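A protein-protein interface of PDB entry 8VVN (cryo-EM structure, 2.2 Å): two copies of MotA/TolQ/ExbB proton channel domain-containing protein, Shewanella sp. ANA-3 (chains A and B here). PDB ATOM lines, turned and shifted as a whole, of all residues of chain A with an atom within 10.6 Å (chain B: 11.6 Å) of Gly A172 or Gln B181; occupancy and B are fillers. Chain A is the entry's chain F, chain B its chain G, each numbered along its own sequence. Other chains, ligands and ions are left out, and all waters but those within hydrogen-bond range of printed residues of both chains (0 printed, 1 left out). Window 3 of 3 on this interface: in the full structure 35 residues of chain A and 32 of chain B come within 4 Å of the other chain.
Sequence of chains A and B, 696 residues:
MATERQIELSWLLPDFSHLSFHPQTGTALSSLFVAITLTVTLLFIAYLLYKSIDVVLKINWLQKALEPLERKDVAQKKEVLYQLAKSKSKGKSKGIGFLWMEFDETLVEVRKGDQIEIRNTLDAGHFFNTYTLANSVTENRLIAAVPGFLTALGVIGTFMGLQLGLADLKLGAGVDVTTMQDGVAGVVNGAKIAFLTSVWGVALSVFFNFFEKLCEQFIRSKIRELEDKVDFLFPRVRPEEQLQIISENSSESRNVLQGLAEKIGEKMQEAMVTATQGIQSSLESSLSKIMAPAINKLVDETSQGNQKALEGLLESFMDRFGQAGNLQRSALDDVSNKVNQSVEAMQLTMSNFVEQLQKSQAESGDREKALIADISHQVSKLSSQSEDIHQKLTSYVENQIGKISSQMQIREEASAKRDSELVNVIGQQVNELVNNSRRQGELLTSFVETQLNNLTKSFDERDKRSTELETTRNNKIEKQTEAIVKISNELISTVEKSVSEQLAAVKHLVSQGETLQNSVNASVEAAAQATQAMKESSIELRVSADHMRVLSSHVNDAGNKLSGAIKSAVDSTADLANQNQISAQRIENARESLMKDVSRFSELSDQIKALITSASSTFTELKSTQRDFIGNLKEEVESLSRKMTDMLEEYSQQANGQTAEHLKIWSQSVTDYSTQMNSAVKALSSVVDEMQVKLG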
ATOM      1  N   ASP A 168     -20.931  -7.937  38.442  1.00  0.00           N
ATOM      2  CA  ASP A 168     -20.779  -6.667  39.138  1.00  0.00           C
ATOM      3  C   ASP A 168     -20.636  -5.482  38.193  1.00  0.00           C
ATOM      4  O   ASP A 168     -20.487  -4.351  38.663  1.00  0.00           O
ATOM      5  CB  ASP A 168     -19.578  -6.730  40.095  1.00  0.00           C
ATOM      6  CG  ASP A 168     -18.253  -6.975  39.379  1.00  0.00           C
ATOM      7  OD1 ASP A 168     -17.897  -6.213  38.455  1.00  0.00           O
ATOM      8  OD2 ASP A 168     -17.561  -7.947  39.751  1.00  0.00           O
ATOM      9  N   LEU A 169     -20.675  -5.708  36.884  1.00  0.00           N
ATOM     10  CA  LEU A 169     -20.540  -4.632  35.908  1.00  0.00           C
ATOM     11  C   LEU A 169     -21.925  -4.045  35.671  1.00  0.00           C
ATOM     12  O   LEU A 169     -22.738  -4.611  34.939  1.00  0.00           O
ATOM     13  CB  LEU A 169     -19.917  -5.145  34.617  1.00  0.00           C
ATOM     14  CG  LEU A 169     -19.764  -4.101  33.512  1.00  0.00           C
ATOM     15  CD1 LEU A 169     -18.816  -3.000  33.961  1.00  0.00           C
ATOM     16  CD2 LEU A 169     -19.274  -4.740  32.230  1.00  0.00           C
ATOM     17  N   LYS A 170     -22.195  -2.907  36.295  1.00  0.00           N
ATOM     18  CA  LYS A 170     -23.504  -2.278  36.229  1.00  0.00           C
ATOM     19  C   LYS A 170     -23.473  -1.160  35.198  1.00  0.00           C
ATOM     20  O   LYS A 170     -22.747  -0.174  35.357  1.00  0.00           O
ATOM     21  CB  LYS A 170     -23.927  -1.755  37.602  1.00  0.00           C
ATOM     22  CG  LYS A 170     -24.175  -2.869  38.610  1.00  0.00           C
ATOM     23  CD  LYS A 170     -24.747  -2.347  39.914  1.00  0.00           C
ATOM     24  CE  LYS A 170     -23.692  -1.630  40.729  1.00  0.00           C
ATOM     25  NZ  LYS A 170     -24.203  -1.207  42.058  1.00  0.00           N
ATOM     26  N   LEU A 171     -24.244  -1.332  34.139  1.00  0.00           N
ATOM     27  CA  LEU A 171     -24.467  -0.323  33.126  1.00  0.00           C
ATOM     28  C   LEU A 171     -25.932   0.098  33.202  1.00  0.00           C
ATOM     29  O   LEU A 171     -26.673  -0.313  34.100  1.00  0.00           O
ATOM     30  CB  LEU A 171     -24.075  -0.866  31.751  1.00  0.00           C
ATOM     31  CG  LEU A 171     -22.632  -1.371  31.641  1.00  0.00           C
ATOM     32  CD1 LEU A 171     -22.441  -2.189  30.381  1.00  0.00           C
ATOM     33  CD2 LEU A 171     -21.639  -0.219  31.688  1.00  0.00           C
ATOM     34  N   GLY A 172     -26.353   0.924  32.267  1.00  0.00           N
ATOM     35  CA  GLY A 172     -27.723   1.382  32.310  1.00  0.00           C
ATOM     36  C   GLY A 172     -27.816   2.850  32.681  1.00  0.00           C
ATOM     37  O   GLY A 172     -26.907   3.437  33.274  1.00  0.00           O
ATOM     38  N   ALA A 173     -28.947   3.445  32.315  1.00  0.00           N
ATOM     39  CA  ALA A 173     -29.143   4.871  32.521  1.00  0.00           C
ATOM     40  C   ALA A 173     -29.072   5.213  34.002  1.00  0.00           C
ATOM     41  O   ALA A 173     -29.689   4.548  34.839  1.00  0.00           O
ATOM     42  CB  ALA A 173     -30.486   5.303  31.937  1.00  0.00           C
ATOM     43  N   GLY A 174     -28.305   6.251  34.325  1.00  0.00           N
ATOM     44  CA  GLY A 174     -28.169   6.718  35.686  1.00  0.00           C
ATOM     45  C   GLY A 174     -26.950   6.212  36.424  1.00  0.00           C
ATOM     46  O   GLY A 174     -26.617   6.765  37.478  1.00  0.00           O
ATOM     47  N   VAL A 175     -26.275   5.182  35.911  1.00  0.00           N
ATOM     48  CA  VAL A 175     -25.079   4.671  36.570  1.00  0.00           C
ATOM     49  C   VAL A 175     -23.935   5.653  36.366  1.00  0.00           C
ATOM     50  O   VAL A 175     -23.635   6.058  35.236  1.00  0.00           O
ATOM     51  CB  VAL A 175     -24.720   3.276  36.037  1.00  0.00           C
ATOM     52  CG1 VAL A 175     -23.360   2.862  36.539  1.00  0.00           C
ATOM     53  CG2 VAL A 175     -25.765   2.262  36.458  1.00  0.00           C
ATOM     54  N   ASP A 176     -23.287   6.037  37.459  1.00  0.00           N
ATOM     55  CA  ASP A 176     -22.266   7.069  37.423  1.00  0.00           C
ATOM     56  C   ASP A 176     -20.879   6.472  37.201  1.00  0.00           C
ATOM     57  O   ASP A 176     -20.689   5.257  37.183  1.00  0.00           O
ATOM     58  CB  ASP A 176     -22.293   7.892  38.708  1.00  0.00           C
ATOM     59  CG  ASP A 176     -22.093   7.048  39.942  1.00  0.00           C
ATOM     60  OD1 ASP A 176     -21.160   7.341  40.714  1.00  0.00           O
ATOM     61  OD2 ASP A 176     -22.867   6.090  40.139  1.00  0.00           O
ATOM     62  N   VAL A 177     -19.900   7.364  37.037  1.00  0.00           N
ATOM     63  CA  VAL A 177     -18.541   6.957  36.693  1.00  0.00           C
ATOM     64  C   VAL A 177     -17.939   6.091  37.790  1.00  0.00           C
ATOM     65  O   VAL A 177     -17.255   5.102  37.510  1.00  0.00           O
ATOM     66  CB  VAL A 177     -17.676   8.199  36.408  1.00  0.00           C
ATOM     67  CG1 VAL A 177     -16.199   7.858  36.445  1.00  0.00           C
ATOM     68  CG2 VAL A 177     -18.043   8.784  35.077  1.00  0.00           C
ATOM     69  N   THR A 179     -19.476   4.063  39.868  1.00  0.00           N
ATOM     70  CA  THR A 179     -20.045   2.725  39.771  1.00  0.00           C
ATOM     71  C   THR A 179     -19.515   1.985  38.549  1.00  0.00           C
ATOM     72  O   THR A 179     -19.190   0.796  38.631  1.00  0.00           O
ATOM     73  CB  THR A 179     -21.571   2.809  39.741  1.00  0.00           C
ATOM     74  OG1 THR A 179     -22.038   3.444  40.937  1.00  0.00           O
ATOM     75  CG2 THR A 179     -22.180   1.428  39.650  1.00  0.00           C
ATOM     76  N   MET A 180     -19.427   2.668  37.404  1.00  0.00           N
ATOM     77  CA  MET A 180     -18.852   2.045  36.216  1.00  0.00           C
ATOM     78  C   MET A 180     -17.395   1.684  36.438  1.00  0.00           C
ATOM     79  O   MET A 180     -16.938   0.617  36.013  1.00  0.00           O
ATOM     80  CB  MET A 180     -18.973   2.972  35.012  1.00  0.00           C
ATOM     81  CG  MET A 180     -20.361   3.449  34.714  1.00  0.00           C
ATOM     82  SD  MET A 180     -20.457   4.308  33.145  1.00  0.00           S
ATOM     83  CE  MET A 180     -21.928   3.549  32.494  1.00  0.00           C
ATOM     84  N   GLN A 181     -16.648   2.570  37.088  1.00  0.00           N
ATOM     85  CA  GLN A 181     -15.228   2.339  37.295  1.00  0.00           C
ATOM     86  C   GLN A 181     -15.002   1.135  38.204  1.00  0.00           C
ATOM     87  O   GLN A 181     -14.086   0.337  37.979  1.00  0.00           O
ATOM     88  CB  GLN A 181     -14.596   3.602  37.872  1.00  0.00           C
ATOM     89  CG  GLN A 181     -13.118   3.551  38.063  1.00  0.00           C
ATOM     90  CD  GLN A 181     -12.366   3.370  36.766  1.00  0.00           C
ATOM     91  OE1 GLN A 181     -11.869   2.283  36.465  1.00  0.00           O
ATOM     92  NE2 GLN A 181     -12.263   4.443  35.994  1.00  0.00           N
ATOM     93  N   GLY B 165     -26.850 -11.498  23.228  1.00  0.00           N
ATOM     94  CA  GLY B 165     -26.058 -10.284  23.340  1.00  0.00           C
ATOM     95  C   GLY B 165     -25.812  -9.626  21.998  1.00  0.00           C
ATOM     96  O   GLY B 165     -25.779  -8.398  21.895  1.00  0.00           O
ATOM     97  N   ALA B 167     -27.906  -9.652  19.497  1.00  0.00           N
ATOM     98  CA  ALA B 167     -29.148  -8.998  19.105  1.00  0.00           C
ATOM     99  C   ALA B 167     -29.324  -7.651  19.788  1.00  0.00           C
ATOM    100  O   ALA B 167     -29.940  -6.746  19.217  1.00  0.00           O
ATOM    101  CB  ALA B 167     -30.340  -9.897  19.422  1.00  0.00           C
ATOM    102  N   ASP B 168     -28.805  -7.501  21.006  1.00  0.00           N
ATOM    103  CA  ASP B 168     -28.998  -6.270  21.761  1.00  0.00           C
ATOM    104  C   ASP B 168     -28.128  -5.125  21.263  1.00  0.00           C
ATOM    105  O   ASP B 168     -28.431  -3.965  21.559  1.00  0.00           O
ATOM    106  CB  ASP B 168     -28.716  -6.520  23.242  1.00  0.00           C
ATOM    107  CG  ASP B 168     -29.853  -7.237  23.933  1.00  0.00           C
ATOM    108  OD1 ASP B 168     -30.992  -6.728  23.885  1.00  0.00           O
ATOM    109  OD2 ASP B 168     -29.608  -8.309  24.525  1.00  0.00           O
ATOM    110  N   LEU B 169     -27.069  -5.425  20.519  1.00  0.00           N
ATOM    111  CA  LEU B 169     -26.157  -4.396  20.042  1.00  0.00           C
ATOM    112  C   LEU B 169     -26.868  -3.389  19.152  1.00  0.00           C
ATOM    113  O   LEU B 169     -27.624  -3.757  18.249  1.00  0.00           O
ATOM    114  CB  LEU B 169     -25.004  -5.042  19.284  1.00  0.00           C
ATOM    115  CG  LEU B 169     -23.915  -5.562  20.205  1.00  0.00           C
ATOM    116  CD1 LEU B 169     -22.831  -6.240  19.421  1.00  0.00           C
ATOM    117  CD2 LEU B 169     -23.344  -4.387  20.981  1.00  0.00           C
ATOM    118  N   LYS B 170     -26.617  -2.113  19.414  1.00  0.00           N
ATOM    119  CA  LYS B 170     -27.144  -1.013  18.616  1.00  0.00           C
ATOM    120  C   LYS B 170     -25.947  -0.318  17.980  1.00  0.00           C
ATOM    121  O   LYS B 170     -25.228   0.433  18.645  1.00  0.00           O
ATOM    122  CB  LYS B 170     -27.970  -0.060  19.471  1.00  0.00           C
ATOM    123  CG  LYS B 170     -28.994  -0.754  20.351  1.00  0.00           C
ATOM    124  CD  LYS B 170     -30.251  -1.077  19.567  1.00  0.00           C
ATOM    125  CE  LYS B 170     -31.433  -1.301  20.490  1.00  0.00           C
ATOM    126  NZ  LYS B 170     -32.173  -0.037  20.764  1.00  0.00           N
ATOM    127  N   LEU B 171     -25.731  -0.582  16.701  1.00  0.00           N
ATOM    128  CA  LEU B 171     -24.599  -0.065  15.952  1.00  0.00           C
ATOM    129  C   LEU B 171     -25.098   0.831  14.824  1.00  0.00           C
ATOM    130  O   LEU B 171     -26.295   1.078  14.677  1.00  0.00           O
ATOM    131  CB  LEU B 171     -23.745  -1.209  15.401  1.00  0.00           C
ATOM    132  CG  LEU B 171     -22.899  -1.984  16.407  1.00  0.00           C
ATOM    133  CD1 LEU B 171     -22.334  -3.231  15.761  1.00  0.00           C
ATOM    134  CD2 LEU B 171     -21.784  -1.108  16.937  1.00  0.00           C
ATOM    135  N   GLY B 172     -24.160   1.308  14.020  1.00  0.00           N
ATOM    136  CA  GLY B 172     -24.466   2.216  12.939  1.00  0.00           C
ATOM    137  C   GLY B 172     -24.205   3.663  13.321  1.00  0.00           C
ATOM    138  O   GLY B 172     -24.082   4.022  14.493  1.00  0.00           O
ATOM    139  N   GLY B 174     -24.947   7.697  13.778  1.00  0.00           N
ATOM    140  CA  GLY B 174     -26.058   8.438  14.352  1.00  0.00           C
ATOM    141  C   GLY B 174     -26.794   7.718  15.460  1.00  0.00           C
ATOM    142  O   GLY B 174     -28.031   7.736  15.491  1.00  0.00           O
ATOM    143  N   VAL B 175     -26.064   7.084  16.374  1.00  0.00           N
ATOM    144  CA  VAL B 175     -26.644   6.399  17.523  1.00  0.00           C
ATOM    145  C   VAL B 175     -26.123   7.075  18.782  1.00  0.00           C
ATOM    146  O   VAL B 175     -24.912   7.275  18.928  1.00  0.00           O
ATOM    147  CB  VAL B 175     -26.309   4.896  17.521  1.00  0.00           C
ATOM    148  CG1 VAL B 175     -26.833   4.233  18.777  1.00  0.00           C
ATOM    149  CG2 VAL B 175     -26.896   4.228  16.292  1.00  0.00           C
ATOM    150  N   ASP B 176     -27.035   7.436  19.680  1.00  0.00           N
ATOM    151  CA  ASP B 176     -26.652   8.160  20.879  1.00  0.00           C
ATOM    152  C   ASP B 176     -25.891   7.248  21.841  1.00  0.00           C
ATOM    153  O   ASP B 176     -25.894   6.021  21.720  1.00  0.00           O
ATOM    154  CB  ASP B 176     -27.883   8.757  21.560  1.00  0.00           C
ATOM    155  CG  ASP B 176     -29.000   7.751  21.729  1.00  0.00           C
ATOM    156  OD1 ASP B 176     -29.672   7.432  20.726  1.00  0.00           O
ATOM    157  OD2 ASP B 176     -29.209   7.280  22.867  1.00  0.00           O
ATOM    158  N   VAL B 177     -25.220   7.879  22.806  1.00  0.00           N
ATOM    159  CA  VAL B 177     -24.409   7.140  23.769  1.00  0.00           C
ATOM    160  C   VAL B 177     -25.281   6.243  24.635  1.00  0.00           C
ATOM    161  O   VAL B 177     -24.920   5.096  24.921  1.00  0.00           O
ATOM    162  CB  VAL B 177     -23.573   8.114  24.616  1.00  0.00           C
ATOM    163  CG1 VAL B 177     -22.996   7.415  25.826  1.00  0.00           C
ATOM    164  CG2 VAL B 177     -22.465   8.704  23.783  1.00  0.00           C
ATOM    165  N   THR B 178     -26.441   6.744  25.066  1.00  0.00           N
ATOM    166  CA  THR B 178     -27.310   5.954  25.933  1.00  0.00           C
ATOM    167  C   THR B 178     -27.786   4.687  25.232  1.00  0.00           C
ATOM    168  O   THR B 178     -27.856   3.618  25.848  1.00  0.00           O
ATOM    169  CB  THR B 178     -28.503   6.792  26.394  1.00  0.00           C
ATOM    170  OG1 THR B 178     -29.473   6.867  25.343  1.00  0.00           O
ATOM    171  CG2 THR B 178     -28.058   8.195  26.759  1.00  0.00           C
ATOM    172  N   THR B 179     -28.119   4.789  23.945  1.00  0.00           N
ATOM    173  CA  THR B 179     -28.550   3.612  23.199  1.00  0.00           C
ATOM    174  C   THR B 179     -27.401   2.625  23.011  1.00  0.00           C
ATOM    175  O   THR B 179     -27.585   1.414  23.172  1.00  0.00           O
ATOM    176  CB  THR B 179     -29.133   4.039  21.853  1.00  0.00           C
ATOM    177  OG1 THR B 179     -30.389   4.698  22.066  1.00  0.00           O
ATOM    178  CG2 THR B 179     -29.373   2.838  20.971  1.00  0.00           C
ATOM    179  N   MET B 180     -26.207   3.124  22.682  1.00  0.00           N
ATOM    180  CA  MET B 180     -25.043   2.248  22.584  1.00  0.00           C
ATOM    181  C   MET B 180     -24.677   1.660  23.940  1.00  0.00           C
ATOM    182  O   MET B 180     -24.235   0.508  24.025  1.00  0.00           O
ATOM    183  CB  MET B 180     -23.862   3.005  21.982  1.00  0.00           C
ATOM    184  CG  MET B 180     -23.911   3.100  20.468  1.00  0.00           C
ATOM    185  SD  MET B 180     -22.566   4.059  19.751  1.00  0.00           S
ATOM    186  CE  MET B 180     -22.557   5.484  20.831  1.00  0.00           C
ATOM    187  N   GLN B 181     -24.844   2.440  25.008  1.00  0.00           N
ATOM    188  CA  GLN B 181     -24.642   1.912  26.352  1.00  0.00           C
ATOM    189  C   GLN B 181     -25.604   0.768  26.644  1.00  0.00           C
ATOM    190  O   GLN B 181     -25.212  -0.250  27.227  1.00  0.00           O
ATOM    191  CB  GLN B 181     -24.814   3.028  27.376  1.00  0.00           C
ATOM    192  CG  GLN B 181     -24.561   2.610  28.799  1.00  0.00           C
ATOM    193  CD  GLN B 181     -24.387   3.790  29.721  1.00  0.00           C
ATOM    194  OE1 GLN B 181     -24.017   4.875  29.289  1.00  0.00           O
ATOM    195  NE2 GLN B 181     -24.650   3.583  31.001  1.00  0.00           N
ATOM    196  N   ASP B 182     -26.870   0.919  26.254  1.00  0.00           N
ATOM    197  CA  ASP B 182     -27.842  -0.148  26.457  1.00  0.00           C
ATOM    198  C   ASP B 182     -27.487  -1.385  25.642  1.00  0.00           C
ATOM    199  O   ASP B 182     -27.679  -2.515  26.103  1.00  0.00           O
ATOM    200  CB  ASP B 182     -29.242   0.349  26.107  1.00  0.00           C
ATOM    201  CG  ASP B 182     -30.327  -0.470  26.766  1.00  0.00           C
ATOM    202  OD1 ASP B 182     -30.388  -0.486  28.012  1.00  0.00           O
ATOM    203  OD2 ASP B 182     -31.120  -1.098  26.037  1.00  0.00           O
ATOM    204  N   GLY B 183     -26.972  -1.191  24.428  1.00  0.00           N
ATOM    205  CA  GLY B 183     -26.519  -2.323  23.640  1.00  0.00           C
ATOM    206  C   GLY B 183     -25.371  -3.068  24.293  1.00  0.00           C
ATOM    207  O   GLY B 183     -25.301  -4.297  24.229  1.00  0.00           O
ATOM    208  N   VAL B 184     -24.451  -2.336  24.922  1.00  0.00           N
ATOM    209  CA  VAL B 184     -23.348  -2.982  25.625  1.00  0.00           C
ATOM    210  C   VAL B 184     -23.863  -3.712  26.858  1.00  0.00           C
ATOM    211  O   VAL B 184     -23.407  -4.815  27.180  1.00  0.00           O
ATOM    212  CB  VAL B 184     -22.263  -1.948  25.980  1.00  0.00           C
ATOM    213  CG1 VAL B 184     -21.300  -2.506  27.010  1.00  0.00           C
ATOM    214  CG2 VAL B 184     -21.524  -1.506  24.739  1.00  0.00           C
ATOM    215  N   ALA B 185     -24.831  -3.117  27.560  1.00  0.00           N
ATOM    216  CA  ALA B 185     -25.453  -3.799  28.689  1.00  0.00           C
ATOM    217  C   ALA B 185     -26.140  -5.085  28.245  1.00  0.00           C
ATOM    218  O   ALA B 185     -26.125  -6.086  28.969  1.00  0.00           O
ATOM    219  CB  ALA B 185     -26.446  -2.868  29.385  1.00  0.00           C
ATOM    220  N   GLY B 186     -26.748  -5.076  27.057  1.00  0.00           N
ATOM    221  CA  GLY B 186     -27.317  -6.299  26.517  1.00  0.00           C
ATOM    222  C   GLY B 186     -26.270  -7.353  26.211  1.00  0.00           C
ATOM    223  O   GLY B 186     -26.499  -8.546  26.424  1.00  0.00           O
ATOM    224  N   VAL B 187     -25.112  -6.930  25.697  1.00  0.00           N
ATOM    225  CA  VAL B 187     -24.010  -7.860  25.459  1.00  0.00           C
ATOM    226  C   VAL B 187     -23.528  -8.461  26.769  1.00  0.00           C
ATOM    227  O   VAL B 187     -23.270  -9.667  26.859  1.00  0.00           O
ATOM    228  CB  VAL B 187     -22.868  -7.154  24.707  1.00  0.00           C
ATOM    229  CG1 VAL B 187     -21.572  -7.932  24.839  1.00  0.00           C
ATOM    230  CG2 VAL B 187     -23.225  -7.026  23.270  1.00  0.00           C
ATOM    231  N   VAL B 188     -23.389  -7.631  27.801  1.00  0.00           N
ATOM    232  CA  VAL B 188     -23.026  -8.139  29.117  1.00  0.00           C
ATOM    233  C   VAL B 188     -24.093  -9.101  29.617  1.00  0.00           C
ATOM    234  O   VAL B 188     -23.785 -10.162  30.174  1.00  0.00           O
ATOM    235  CB  VAL B 188     -22.800  -6.969  30.094  1.00  0.00           C
ATOM    236  CG1 VAL B 188     -22.759  -7.459  31.528  1.00  0.00           C
ATOM    237  CG2 VAL B 188     -21.523  -6.230  29.735  1.00  0.00           C
ATOM    238  N   ASN B 189     -25.364  -8.757  29.401  1.00  0.00           N
ATOM    239  CA  ASN B 189     -26.459  -9.623  29.819  1.00  0.00           C
ATOM    240  C   ASN B 189     -26.407 -10.969  29.108  1.00  0.00           C
ATOM    241  O   ASN B 189     -26.584 -12.018  29.735  1.00  0.00           O
ATOM    242  CB  ASN B 189     -27.791  -8.925  29.556  1.00  0.00           C
ATOM    243  CG  ASN B 189     -28.950  -9.608  30.232  1.00  0.00           C
ATOM    244  OD1 ASN B 189     -29.865 -10.096  29.576  1.00  0.00           O
ATOM    245  ND2 ASN B 189     -28.922  -9.646  31.555  1.00  0.00           N
ATOM    246  N   GLY B 190     -26.157 -10.961  27.798  1.00  0.00           N
ATOM    247  CA  GLY B 190     -26.052 -12.212  27.068  1.00  0.00           C
ATOM    248  C   GLY B 190     -24.849 -13.034  27.487  1.00  0.00           C
ATOM    249  O   GLY B 190     -24.935 -14.258  27.609  1.00  0.00           O
ATOM    250  N   LYS B 192     -23.491 -13.101  30.417  1.00  0.00           N
ATOM    251  CA  LYS B 192     -23.769 -13.720  31.710  1.00  0.00           C
ATOM    252  C   LYS B 192     -24.592 -14.993  31.557  1.00  0.00           C
ATOM    253  O   LYS B 192     -24.367 -15.968  32.281  1.00  0.00           O
ATOM    254  CB  LYS B 192     -24.473 -12.739  32.646  1.00  0.00           C
ATOM    255  CG  LYS B 192     -23.637 -11.540  33.037  1.00  0.00           C
ATOM    256  CD  LYS B 192     -24.300 -10.759  34.157  1.00  0.00           C
ATOM    257  CE  LYS B 192     -25.074  -9.569  33.632  1.00  0.00           C
ATOM    258  NZ  LYS B 192     -25.046  -8.437  34.599  1.00  0.00           N
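The backbone carbonyl oxygen (O) of Gly A172 sits at hydrogen-bond distance from the side-chain amide nitrogen (NE2) of Gln B181, 3.2 Å away.
Among the printed residues, merely in contact across the chains: Met A180 with Gln B181 (3.1 Å), Leu A171 with Val B184 (3.6 Å), Leu A169 with Val B188 (3.7 Å) and Leu A171 with Ala B185 (3.8 Å).
Printed residues of chain B within 4 Å of Leu A169: Val B188. Leu A171 touches just these residues of chain B: Val B184 and Ala B185. Of chain B, only Gln B181 (3.2 Å) comes within 4 Å of Gly A172. No residue of chain B comes within 4 Å of Ala A173. No residue of chain B comes within 4 Å of Val A175. Of the printed residues of chain B, Met A180 touches Gln B181. No residue of chain A comes within 4 Å of Thr B178. Of chain A, only Gly A172 (3.2 Å) and Met A180 (3.1 Å) come within 4 Å of Gln B181. Asp B182 touches none of the printed residues of chain A. No residue of chain A comes within 4 Å of Gly B183. Of chain A, only Leu A171 (3.6 Å) comes within 4 Å of Val B184. Of chain A, only Leu A171 (3.8 Å) comes within 4 Å of Ala B185. Of the printed residues of chain A, Val B188 touches Leu A169. The nearest residue of chain A that does not touch Gln B181 is Leu A171 (4.3 Å).
Of the 13 printed residues of chain A, 4 touch a printed residue of chain B. Printed residues of chain A that touch a printed residue of chain B: Leu A169, Leu A171, Gly A172 and Met A180. Hydrophobic or aromatic side chains of chain B that line the printed part of chain A: Val B184, Ala B185 and Val B188. Among the printed residues, 5 pairs touch across the chains. Among the printed residues, no Asp or Glu carboxylate lies within 4 Å of a Lys or Arg side-chain nitrogen of the other chain.
Gly A172 touches Gln B181, but with the chains exchanged Gln A181 does not touch Gly B172 (23.8 Å). Met A180 touches Gln B181, but with the chains exchanged Gln A181 does not touch Met B180 (15.2 Å). 12 positions are printed for both chains. Of the 5 pairs that touch across the chains among the printed residues, none has its exchanged pair printed and touching as well.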
